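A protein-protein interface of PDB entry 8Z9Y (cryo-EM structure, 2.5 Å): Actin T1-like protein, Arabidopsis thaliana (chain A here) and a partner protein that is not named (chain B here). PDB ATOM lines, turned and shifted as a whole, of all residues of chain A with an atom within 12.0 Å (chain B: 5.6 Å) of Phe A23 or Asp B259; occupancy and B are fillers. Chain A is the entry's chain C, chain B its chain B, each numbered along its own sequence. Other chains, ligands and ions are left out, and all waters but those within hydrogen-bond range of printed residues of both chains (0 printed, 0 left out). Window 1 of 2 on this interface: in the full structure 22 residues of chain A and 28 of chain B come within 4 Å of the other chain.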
ATOM      1  N   ASN A   7      17.908   9.648   4.309  1.00  0.00           N
ATOM      2  CA  ASN A   7      18.070   9.058   2.987  1.00  0.00           C
ATOM      3  C   ASN A   7      16.912   9.437   2.069  1.00  0.00           C
ATOM      4  O   ASN A   7      16.297  10.491   2.233  1.00  0.00           O
ATOM      5  CB  ASN A   7      18.191   7.536   3.094  1.00  0.00           C
ATOM      6  CG  ASN A   7      16.960   6.895   3.707  1.00  0.00           C
ATOM      7  OD1 ASN A   7      16.733   6.991   4.912  1.00  0.00           O
ATOM      8  ND2 ASN A   7      16.164   6.231   2.879  1.00  0.00           N
ATOM      9  N   ALA A   8      16.621   8.572   1.100  1.00  0.00           N
ATOM     10  CA  ALA A   8      15.572   8.809   0.118  1.00  0.00           C
ATOM     11  C   ALA A   8      14.543   7.692   0.202  1.00  0.00           C
ATOM     12  O   ALA A   8      14.897   6.511   0.137  1.00  0.00           O
ATOM     13  CB  ALA A   8      16.151   8.891  -1.295  1.00  0.00           C
ATOM     14  N   TYR A   9      13.273   8.068   0.349  1.00  0.00           N
ATOM     15  CA  TYR A   9      12.169   7.129   0.229  1.00  0.00           C
ATOM     16  C   TYR A   9      11.159   7.528  -0.835  1.00  0.00           C
ATOM     17  O   TYR A   9      10.239   6.749  -1.111  1.00  0.00           O
ATOM     18  CB  TYR A   9      11.458   6.952   1.579  1.00  0.00           C
ATOM     19  CG  TYR A   9      11.924   5.724   2.327  1.00  0.00           C
ATOM     20  CD1 TYR A   9      13.003   5.786   3.198  1.00  0.00           C
ATOM     21  CD2 TYR A   9      11.293   4.499   2.154  1.00  0.00           C
ATOM     22  CE1 TYR A   9      13.439   4.665   3.877  1.00  0.00           C
ATOM     23  CE2 TYR A   9      11.720   3.372   2.832  1.00  0.00           C
ATOM     24  CZ  TYR A   9      12.794   3.460   3.691  1.00  0.00           C
ATOM     25  OH  TYR A   9      13.222   2.342   4.368  1.00  0.00           O
ATOM     26  N   ASP A  12      15.479  12.016  -4.255  1.00  0.00           N
ATOM     27  CA  ASP A  12      16.231  13.262  -4.331  1.00  0.00           C
ATOM     28  C   ASP A  12      17.624  12.956  -4.872  1.00  0.00           C
ATOM     29  O   ASP A  12      18.371  12.177  -4.269  1.00  0.00           O
ATOM     30  CB  ASP A  12      16.299  13.958  -2.968  1.00  0.00           C
ATOM     31  CG  ASP A  12      16.445  12.986  -1.816  1.00  0.00           C
ATOM     32  OD1 ASP A  12      16.865  11.836  -2.051  1.00  0.00           O
ATOM     33  OD2 ASP A  12      16.137  13.373  -0.669  1.00  0.00           O
ATOM     34  N   GLY A  14      20.683  14.756  -5.667  1.00  0.00           N
ATOM     35  CA  GLY A  14      21.946  15.217  -5.127  1.00  0.00           C
ATOM     36  C   GLY A  14      21.832  16.295  -4.071  1.00  0.00           C
ATOM     37  O   GLY A  14      22.811  16.991  -3.789  1.00  0.00           O
ATOM     38  N   VAL A  15      20.648  16.454  -3.488  1.00  0.00           N
ATOM     39  CA  VAL A  15      20.505  17.462  -2.430  1.00  0.00           C
ATOM     40  C   VAL A  15      21.324  17.026  -1.222  1.00  0.00           C
ATOM     41  O   VAL A  15      21.158  15.888  -0.740  1.00  0.00           O
ATOM     42  CB  VAL A  15      19.025  17.652  -2.058  1.00  0.00           C
ATOM     43  CG1 VAL A  15      18.889  18.678  -0.943  1.00  0.00           C
ATOM     44  CG2 VAL A  15      18.221  18.072  -3.278  1.00  0.00           C
ATOM     45  N   PRO A  16      22.217  17.867  -0.702  1.00  0.00           N
ATOM     46  CA  PRO A  16      23.129  17.414   0.353  1.00  0.00           C
ATOM     47  C   PRO A  16      22.392  17.053   1.632  1.00  0.00           C
ATOM     48  O   PRO A  16      21.326  17.590   1.940  1.00  0.00           O
ATOM     49  CB  PRO A  16      24.056  18.619   0.566  1.00  0.00           C
ATOM     50  CG  PRO A  16      23.880  19.476  -0.649  1.00  0.00           C
ATOM     51  CD  PRO A  16      22.472  19.261  -1.098  1.00  0.00           C
ATOM     52  N   HIS A  17      22.977  16.118   2.375  1.00  0.00           N
ATOM     53  CA  HIS A  17      22.486  15.724   3.688  1.00  0.00           C
ATOM     54  C   HIS A  17      23.422  16.284   4.749  1.00  0.00           C
ATOM     55  O   HIS A  17      24.644  16.126   4.649  1.00  0.00           O
ATOM     56  CB  HIS A  17      22.389  14.202   3.809  1.00  0.00           C
ATOM     57  CG  HIS A  17      21.053  13.652   3.419  1.00  0.00           C
ATOM     58  ND1 HIS A  17      20.344  12.782   4.219  1.00  0.00           N
ATOM     59  CD2 HIS A  17      20.295  13.850   2.315  1.00  0.00           C
ATOM     60  CE1 HIS A  17      19.207  12.467   3.624  1.00  0.00           C
ATOM     61  NE2 HIS A  17      19.153  13.102   2.468  1.00  0.00           N
ATOM     62  N   ALA A  18      22.848  16.943   5.751  1.00  0.00           N
ATOM     63  CA  ALA A  18      23.650  17.595   6.775  1.00  0.00           C
ATOM     64  C   ALA A  18      24.468  16.576   7.557  1.00  0.00           C
ATOM     65  O   ALA A  18      24.000  15.476   7.860  1.00  0.00           O
ATOM     66  CB  ALA A  18      22.751  18.383   7.726  1.00  0.00           C
ATOM     67  N   ASP A  19      25.703  16.950   7.878  1.00  0.00           N
ATOM     68  CA  ASP A  19      26.555  16.093   8.691  1.00  0.00           C
ATOM     69  C   ASP A  19      26.027  16.045  10.119  1.00  0.00           C
ATOM     70  O   ASP A  19      25.744  17.084  10.725  1.00  0.00           O
ATOM     71  CB  ASP A  19      27.996  16.597   8.660  1.00  0.00           C
ATOM     72  CG  ASP A  19      28.086  18.108   8.725  1.00  0.00           C
ATOM     73  OD1 ASP A  19      27.062  18.774   8.468  1.00  0.00           O
ATOM     74  OD2 ASP A  19      29.178  18.629   9.033  1.00  0.00           O
ATOM     75  N   ALA A  20      25.897  14.832  10.658  1.00  0.00           N
ATOM     76  CA  ALA A  20      25.239  14.646  11.947  1.00  0.00           C
ATOM     77  C   ALA A  20      26.098  15.088  13.124  1.00  0.00           C
ATOM     78  O   ALA A  20      25.558  15.322  14.210  1.00  0.00           O
ATOM     79  CB  ALA A  20      24.838  13.182  12.124  1.00  0.00           C
ATOM     80  N   ASP A  21      27.415  15.207  12.942  1.00  0.00           N
ATOM     81  CA  ASP A  21      28.286  15.529  14.067  1.00  0.00           C
ATOM     82  C   ASP A  21      28.060  16.936  14.601  1.00  0.00           C
ATOM     83  O   ASP A  21      28.501  17.236  15.714  1.00  0.00           O
ATOM     84  CB  ASP A  21      29.753  15.361  13.668  1.00  0.00           C
ATOM     85  CG  ASP A  21      30.026  15.811  12.251  1.00  0.00           C
ATOM     86  OD1 ASP A  21      29.053  16.115  11.533  1.00  0.00           O
ATOM     87  OD2 ASP A  21      31.209  15.863  11.856  1.00  0.00           O
ATOM     88  N   ARG A  22      27.383  17.801  13.844  1.00  0.00           N
ATOM     89  CA  ARG A  22      27.149  19.166  14.304  1.00  0.00           C
ATOM     90  C   ARG A  22      26.217  19.194  15.508  1.00  0.00           C
ATOM     91  O   ARG A  22      26.508  19.843  16.520  1.00  0.00           O
ATOM     92  CB  ARG A  22      26.576  20.000  13.162  1.00  0.00           C
ATOM     93  CG  ARG A  22      27.439  19.982  11.928  1.00  0.00           C
ATOM     94  CD  ARG A  22      27.099  21.128  11.009  1.00  0.00           C
ATOM     95  NE  ARG A  22      25.800  20.980  10.369  1.00  0.00           N
ATOM     96  CZ  ARG A  22      25.560  21.287   9.101  1.00  0.00           C
ATOM     97  NH1 ARG A  22      26.513  21.755   8.312  1.00  0.00           N
ATOM     98  NH2 ARG A  22      24.335  21.122   8.616  1.00  0.00           N
ATOM     99  N   PHE A  23      25.084  18.498  15.413  1.00  0.00           N
ATOM    100  CA  PHE A  23      24.137  18.477  16.522  1.00  0.00           C
ATOM    101  C   PHE A  23      24.712  17.727  17.716  1.00  0.00           C
ATOM    102  O   PHE A  23      24.463  18.099  18.870  1.00  0.00           O
ATOM    103  CB  PHE A  23      22.822  17.857  16.060  1.00  0.00           C
ATOM    104  CG  PHE A  23      22.263  18.493  14.820  1.00  0.00           C
ATOM    105  CD1 PHE A  23      21.487  19.636  14.901  1.00  0.00           C
ATOM    106  CD2 PHE A  23      22.521  17.952  13.572  1.00  0.00           C
ATOM    107  CE1 PHE A  23      20.975  20.223  13.761  1.00  0.00           C
ATOM    108  CE2 PHE A  23      22.013  18.536  12.429  1.00  0.00           C
ATOM    109  CZ  PHE A  23      21.239  19.674  12.524  1.00  0.00           C
ATOM    110  N   VAL A  24      25.489  16.673  17.456  1.00  0.00           N
ATOM    111  CA  VAL A  24      26.181  15.973  18.534  1.00  0.00           C
ATOM    112  C   VAL A  24      27.136  16.919  19.248  1.00  0.00           C
ATOM    113  O   VAL A  24      27.201  16.944  20.483  1.00  0.00           O
ATOM    114  CB  VAL A  24      26.919  14.740  17.981  1.00  0.00           C
ATOM    115  CG1 VAL A  24      27.692  14.042  19.087  1.00  0.00           C
ATOM    116  CG2 VAL A  24      25.939  13.784  17.327  1.00  0.00           C
ATOM    117  N   ASN A  25      27.889  17.711  18.483  1.00  0.00           N
ATOM    118  CA  ASN A  25      28.798  18.680  19.084  1.00  0.00           C
ATOM    119  C   ASN A  25      28.039  19.711  19.903  1.00  0.00           C
ATOM    120  O   ASN A  25      28.472  20.086  20.995  1.00  0.00           O
ATOM    121  CB  ASN A  25      29.628  19.366  17.999  1.00  0.00           C
ATOM    122  CG  ASN A  25      30.706  18.469  17.435  1.00  0.00           C
ATOM    123  OD1 ASN A  25      31.107  17.492  18.065  1.00  0.00           O
ATOM    124  ND2 ASN A  25      31.186  18.798  16.242  1.00  0.00           N
ATOM    125  N   ILE A  26      26.900  20.180  19.389  1.00  0.00           N
ATOM    126  CA  ILE A  26      26.106  21.170  20.115  1.00  0.00           C
ATOM    127  C   ILE A  26      25.632  20.602  21.448  1.00  0.00           C
ATOM    128  O   ILE A  26      25.752  21.245  22.498  1.00  0.00           O
ATOM    129  CB  ILE A  26      24.925  21.644  19.250  1.00  0.00           C
ATOM    130  CG1 ILE A  26      25.410  22.596  18.158  1.00  0.00           C
ATOM    131  CG2 ILE A  26      23.864  22.307  20.111  1.00  0.00           C
ATOM    132  CD1 ILE A  26      24.396  22.838  17.065  1.00  0.00           C
ATOM    133  N   TRP A  27      25.093  19.382  21.424  1.00  0.00           N
ATOM    134  CA  TRP A  27      24.588  18.771  22.651  1.00  0.00           C
ATOM    135  C   TRP A  27      25.712  18.506  23.648  1.00  0.00           C
ATOM    136  O   TRP A  27      25.561  18.767  24.851  1.00  0.00           O
ATOM    137  CB  TRP A  27      23.841  17.480  22.319  1.00  0.00           C
ATOM    138  CG  TRP A  27      22.702  17.682  21.364  1.00  0.00           C
ATOM    139  CD1 TRP A  27      22.050  18.852  21.102  1.00  0.00           C
ATOM    140  CD2 TRP A  27      22.085  16.686  20.539  1.00  0.00           C
ATOM    141  NE1 TRP A  27      21.064  18.646  20.169  1.00  0.00           N
ATOM    142  CE2 TRP A  27      21.065  17.325  19.807  1.00  0.00           C
ATOM    143  CE3 TRP A  27      22.294  15.318  20.350  1.00  0.00           C
ATOM    144  CZ2 TRP A  27      20.257  16.642  18.902  1.00  0.00           C
ATOM    145  CZ3 TRP A  27      21.491  14.642  19.450  1.00  0.00           C
ATOM    146  CH2 TRP A  27      20.486  15.305  18.738  1.00  0.00           C
ATOM    147  N   ILE A  28      26.847  17.994  23.166  1.00  0.00           N
ATOM    148  CA  ILE A  28      27.977  17.722  24.048  1.00  0.00           C
ATOM    149  C   ILE A  28      28.497  19.015  24.658  1.00  0.00           C
ATOM    150  O   ILE A  28      28.831  19.067  25.848  1.00  0.00           O
ATOM    151  CB  ILE A  28      29.080  16.967  23.283  1.00  0.00           C
ATOM    152  CG1 ILE A  28      28.634  15.537  22.980  1.00  0.00           C
ATOM    153  CG2 ILE A  28      30.376  16.956  24.077  1.00  0.00           C
ATOM    154  CD1 ILE A  28      29.639  14.743  22.180  1.00  0.00           C
ATOM    155  N   GLY A  29      28.572  20.079  23.858  1.00  0.00           N
ATOM    156  CA  GLY A  29      29.017  21.357  24.383  1.00  0.00           C
ATOM    157  C   GLY A  29      28.070  21.919  25.421  1.00  0.00           C
ATOM    158  O   GLY A  29      28.504  22.493  26.420  1.00  0.00           O
ATOM    159  N   SER A  30      26.762  21.765  25.202  1.00  0.00           N
ATOM    160  CA  SER A  30      25.796  22.225  26.197  1.00  0.00           C
ATOM    161  C   SER A  30      25.951  21.466  27.509  1.00  0.00           C
ATOM    162  O   SER A  30      25.956  22.069  28.592  1.00  0.00           O
ATOM    163  CB  SER A  30      24.375  22.080  25.655  1.00  0.00           C
ATOM    164  OG  SER A  30      24.080  23.107  24.724  1.00  0.00           O
ATOM    165  N   ALA A  31      26.093  20.139  27.433  1.00  0.00           N
ATOM    166  CA  ALA A  31      26.278  19.352  28.649  1.00  0.00           C
ATOM    167  C   ALA A  31      27.571  19.730  29.363  1.00  0.00           C
ATOM    168  O   ALA A  31      27.597  19.870  30.595  1.00  0.00           O
ATOM    169  CB  ALA A  31      26.263  17.860  28.317  1.00  0.00           C
ATOM    170  N   ALA A  32      28.656  19.907  28.604  1.00  0.00           N
ATOM    171  CA  ALA A  32      29.930  20.280  29.203  1.00  0.00           C
ATOM    172  C   ALA A  32      29.857  21.659  29.842  1.00  0.00           C
ATOM    173  O   ALA A  32      30.436  21.886  30.909  1.00  0.00           O
ATOM    174  CB  ALA A  32      31.039  20.231  28.152  1.00  0.00           C
ATOM    175  N   PHE B 198      10.032  17.924   3.825  1.00  0.00           N
ATOM    176  CA  PHE B 198      10.928  17.395   4.845  1.00  0.00           C
ATOM    177  C   PHE B 198      11.190  18.430   5.929  1.00  0.00           C
ATOM    178  O   PHE B 198      11.156  18.111   7.121  1.00  0.00           O
ATOM    179  CB  PHE B 198      12.241  16.939   4.207  1.00  0.00           C
ATOM    180  CG  PHE B 198      13.243  16.407   5.192  1.00  0.00           C
ATOM    181  CD1 PHE B 198      14.131  17.255   5.833  1.00  0.00           C
ATOM    182  CD2 PHE B 198      13.294  15.054   5.480  1.00  0.00           C
ATOM    183  CE1 PHE B 198      15.048  16.766   6.736  1.00  0.00           C
ATOM    184  CE2 PHE B 198      14.211  14.561   6.383  1.00  0.00           C
ATOM    185  CZ  PHE B 198      15.089  15.417   7.011  1.00  0.00           C
ATOM    186  N   THR B 244      20.205  23.769  18.331  1.00  0.00           N
ATOM    187  CA  THR B 244      19.728  22.809  17.341  1.00  0.00           C
ATOM    188  C   THR B 244      18.748  23.466  16.378  1.00  0.00           C
ATOM    189  O   THR B 244      18.827  23.262  15.160  1.00  0.00           O
ATOM    190  CB  THR B 244      19.076  21.616  18.041  1.00  0.00           C
ATOM    191  OG1 THR B 244      20.084  20.830  18.688  1.00  0.00           O
ATOM    192  CG2 THR B 244      18.329  20.747  17.041  1.00  0.00           C
ATOM    193  N   GLU B 247      20.733  25.777  14.068  1.00  0.00           N
ATOM    194  CA  GLU B 247      21.480  25.045  13.053  1.00  0.00           C
ATOM    195  C   GLU B 247      20.552  24.450  12.002  1.00  0.00           C
ATOM    196  O   GLU B 247      20.918  24.374  10.825  1.00  0.00           O
ATOM    197  CB  GLU B 247      22.334  23.960  13.711  1.00  0.00           C
ATOM    198  CG  GLU B 247      22.807  22.887  12.758  1.00  0.00           C
ATOM    199  CD  GLU B 247      23.771  23.426  11.726  1.00  0.00           C
ATOM    200  OE1 GLU B 247      24.586  24.306  12.072  1.00  0.00           O
ATOM    201  OE2 GLU B 247      23.698  22.984  10.562  1.00  0.00           O
ATOM    202  N   SER B 248      19.344  24.039  12.398  1.00  0.00           N
ATOM    203  CA  SER B 248      18.358  23.605  11.413  1.00  0.00           C
ATOM    204  C   SER B 248      17.970  24.750  10.485  1.00  0.00           C
ATOM    205  O   SER B 248      17.804  24.552   9.273  1.00  0.00           O
ATOM    206  CB  SER B 248      17.125  23.041  12.117  1.00  0.00           C
ATOM    207  OG  SER B 248      17.486  22.355  13.301  1.00  0.00           O
ATOM    208  N   CYS B 251      20.766  25.140   8.060  1.00  0.00           N
ATOM    209  CA  CYS B 251      20.706  24.082   7.057  1.00  0.00           C
ATOM    210  C   CYS B 251      19.641  24.377   6.012  1.00  0.00           C
ATOM    211  O   CYS B 251      19.854  24.154   4.814  1.00  0.00           O
ATOM    212  CB  CYS B 251      20.432  22.738   7.729  1.00  0.00           C
ATOM    213  SG  CYS B 251      21.909  21.826   8.197  1.00  0.00           S
ATOM    214  N   TYR B 257      19.166  19.332   3.554  1.00  0.00           N
ATOM    215  CA  TYR B 257      18.374  18.782   4.644  1.00  0.00           C
ATOM    216  C   TYR B 257      19.030  19.079   5.992  1.00  0.00           C
ATOM    217  O   TYR B 257      20.128  19.635   6.081  1.00  0.00           O
ATOM    218  CB  TYR B 257      18.191  17.275   4.474  1.00  0.00           C
ATOM    219  CG  TYR B 257      17.481  16.851   3.209  1.00  0.00           C
ATOM    220  CD1 TYR B 257      18.193  16.497   2.073  1.00  0.00           C
ATOM    221  CD2 TYR B 257      16.096  16.795   3.156  1.00  0.00           C
ATOM    222  CE1 TYR B 257      17.545  16.099   0.920  1.00  0.00           C
ATOM    223  CE2 TYR B 257      15.440  16.404   2.008  1.00  0.00           C
ATOM    224  CZ  TYR B 257      16.168  16.059   0.893  1.00  0.00           C
ATOM    225  OH  TYR B 257      15.518  15.668  -0.254  1.00  0.00           O
ATOM    226  N   ALA B 258      18.337  18.687   7.061  1.00  0.00           N
ATOM    227  CA  ALA B 258      18.820  18.827   8.436  1.00  0.00           C
ATOM    228  C   ALA B 258      18.651  17.468   9.109  1.00  0.00           C
ATOM    229  O   ALA B 258      17.607  17.181   9.699  1.00  0.00           O
ATOM    230  CB  ALA B 258      18.073  19.929   9.178  1.00  0.00           C
ATOM    231  N   ASP B 259      19.685  16.633   9.016  1.00  0.00           N
ATOM    232  CA  ASP B 259      19.646  15.274   9.556  1.00  0.00           C
ATOM    233  C   ASP B 259      20.184  15.290  10.985  1.00  0.00           C
ATOM    234  O   ASP B 259      21.362  15.040  11.243  1.00  0.00           O
ATOM    235  CB  ASP B 259      20.446  14.326   8.671  1.00  0.00           C
ATOM    236  CG  ASP B 259      19.606  13.684   7.584  1.00  0.00           C
ATOM    237  OD1 ASP B 259      18.631  12.979   7.919  1.00  0.00           O
ATOM    238  OD2 ASP B 259      19.920  13.883   6.392  1.00  0.00           O
ATOM    239  N   ILE B 260      19.298  15.591  11.931  1.00  0.00           N
ATOM    240  CA  ILE B 260      19.670  15.490  13.341  1.00  0.00           C
ATOM    241  C   ILE B 260      19.841  14.003  13.637  1.00  0.00           C
ATOM    242  O   ILE B 260      19.133  13.174  13.048  1.00  0.00           O
ATOM    243  CB  ILE B 260      18.645  16.170  14.268  1.00  0.00           C
ATOM    244  CG1 ILE B 260      17.218  15.763  13.935  1.00  0.00           C
ATOM    245  CG2 ILE B 260      18.740  17.670  14.152  1.00  0.00           C
ATOM    246  CD1 ILE B 260      16.339  15.619  15.146  1.00  0.00           C
ATOM    247  N   PRO B 261      20.767  13.622  14.521  1.00  0.00           N
ATOM    248  CA  PRO B 261      21.248  12.230  14.550  1.00  0.00           C
ATOM    249  C   PRO B 261      20.189  11.157  14.757  1.00  0.00           C
ATOM    250  O   PRO B 261      20.050  10.260  13.919  1.00  0.00           O
ATOM    251  CB  PRO B 261      22.239  12.234  15.721  1.00  0.00           C
ATOM    252  CG  PRO B 261      22.677  13.640  15.850  1.00  0.00           C
ATOM    253  CD  PRO B 261      21.523  14.493  15.436  1.00  0.00           C
ATOM    254  N   CYS B 264      15.597  12.023  13.349  1.00  0.00           N
ATOM    255  CA  CYS B 264      15.267  12.630  12.064  1.00  0.00           C
ATOM    256  C   CYS B 264      15.037  11.599  10.974  1.00  0.00           C
ATOM    257  O   CYS B 264      13.914  11.462  10.488  1.00  0.00           O
ATOM    258  CB  CYS B 264      16.367  13.577  11.599  1.00  0.00           C
ATOM    259  SG  CYS B 264      16.342  13.884   9.824  1.00  0.00           S
ATOM    260  N   ASP B 265      16.085  10.858  10.604  1.00  0.00           N
ATOM    261  CA  ASP B 265      16.019  10.003   9.424  1.00  0.00           C
ATOM    262  C   ASP B 265      14.783   9.113   9.454  1.00  0.00           C
ATOM    263  O   ASP B 265      13.856   9.286   8.655  1.00  0.00           O
ATOM    264  CB  ASP B 265      17.293   9.160   9.324  1.00  0.00           C
ATOM    265  CG  ASP B 265      18.536  10.003   9.117  1.00  0.00           C
ATOM    266  OD1 ASP B 265      19.046  10.567  10.107  1.00  0.00           O
ATOM    267  OD2 ASP B 265      19.004  10.101   7.964  1.00  0.00           O
ATOM    268  N   ILE B 269      11.335  10.528   7.836  1.00  0.00           N
ATOM    269  CA  ILE B 269      11.434  10.170   6.428  1.00  0.00           C
ATOM    270  C   ILE B 269      10.514   8.987   6.150  1.00  0.00           C
ATOM    271  O   ILE B 269       9.972   8.853   5.046  1.00  0.00           O
ATOM    272  CB  ILE B 269      12.899   9.877   6.045  1.00  0.00           C
ATOM    273  CG1 ILE B 269      13.593  11.167   5.607  1.00  0.00           C
ATOM    274  CG2 ILE B 269      12.996   8.828   4.950  1.00  0.00           C
ATOM    275  CD1 ILE B 269      15.085  11.031   5.415  1.00  0.00           C
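The side-chain sulfur (SG) of Cys B264 lies within hydrogen-bond range of the side-chain carboxylate (OD1) of Asp B259 (3.1 Å). O of Thr B244 lies within hydrogen-bond range of OG of Ser B248 (2.5 Å). OE2 of Glu B247 sits at hydrogen-bond distance from SG of Cys B251. NH1 of Arg A22 is in salt-bridge range of OD1 of Asp A19 (3.0 Å). The side-chain sulfur (SG) of Cys B251 sits close to the backbone carbonyl oxygen (O) of Tyr B257.
Asp B265 touches Asn A7 (OD2 to N, 3.8 Å). Asn A7 touches Ile B269 (N to CD1, 3.3 Å). His A17 touches Tyr B257. Asp B259 touches Ala A18 (N to CB, 3.8 Å). Ala A20 touches Pro B261 (O to CG, 3.7 Å). CD1 of Phe A23 touches CG2 of Thr B244, at 3.97 Å. Asp B259 touches Phe A23. Pro B261 touches Phe A23 (CD to CB, 3.7 Å). Val A24 touches Pro B261 (CG2 to CG, 3.6 Å). Trp A27 touches Pro B261.
NH2 of Arg A22 is in hydrogen-bond range of SG of Cys B251 (2.6 Å). O of Pro A16 lies within hydrogen-bond range of N of Tyr B257. The side-chain carboxylate (OE2) of Glu B247 lies within salt-bridge range of the guanidinium group (NH2) of Arg A22 (2.8 Å). The side-chain hydroxyl (OG1) of Thr B244 lies within hydrogen-bond range of the indole nitrogen (NE1) of Trp A27 (2.8 Å). The side-chain carboxylate (OD2) of Asp B259 sits at hydrogen-bond distance from a ring nitrogen (ND1) of His A17. OH of Tyr B257 lies within hydrogen-bond range of OD2 of Asp A12, at 2.4 Å.
Of the 23 printed residues of chain A, 12 touch a printed residue of chain B. Hydrophobic or aromatic side chains of chain A that line the printed part of chain B: Tyr A9, Val A15, His A17, Ala A18, Phe A23, Val A24 and Trp A27. Of the 13 printed residues of chain B, 9 touch a printed residue of chain A. Hydrophobic or aromatic side chains of chain B within 4 Å of the printed part of chain A: Tyr B257, Ile B260, Pro B261 and Ile B269. Along chain B the printed residues that touch a printed residue of chain A span positions 244 to 269. Among the printed residues, 23 pairs touch across the chains. Among the printed residues, Asp or Glu carboxylates within 4 Å of a Lys or Arg side-chain nitrogen of the other chain: Arg A22 with Glu B247 (2.8 Å).
Of chain B, only Thr B244 (3.97 Å), Glu B247 (3.4 Å), Asp B259 (3.7 Å), Ile B260 (3.4 Å) and Pro B261 (3.7 Å) come within 4 Å of Phe A23. Asp B259 touches just these residues of chain A: His A17, Ala A18, Ala A20 and Phe A23. No residue of chain A comes within 4 Å of Ser B248. Ile B260 touches one residue of chain A. Pro B261 touches just these residues of chain A: Ala A20 (3.7 Å), Phe A23 (3.7 Å), Val A24 (3.6 Å) and Trp A27 (3.6 Å). Of chain A, only Asn A7 (3.8 Å) comes within 4 Å of Asp B265. Printed residues of chain B within 4 Å of Tyr A9: Ile B269. Of the printed residues of chain B, Asp A12 touches Tyr B257 (2.4 Å). Printed residues of chain B within 4 Å of Ala A20: Asp B259 and Pro B261. The nearest residue of chain B that does not touch Phe A23 is Ser B248 (4.1 Å). The nearest residue of chain A that does not touch Asp B259 is Asp A19 (4.9 Å). The nearest printed residue of chain B that does not touch Pro A16 is Asp B259 (6.0 Å).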
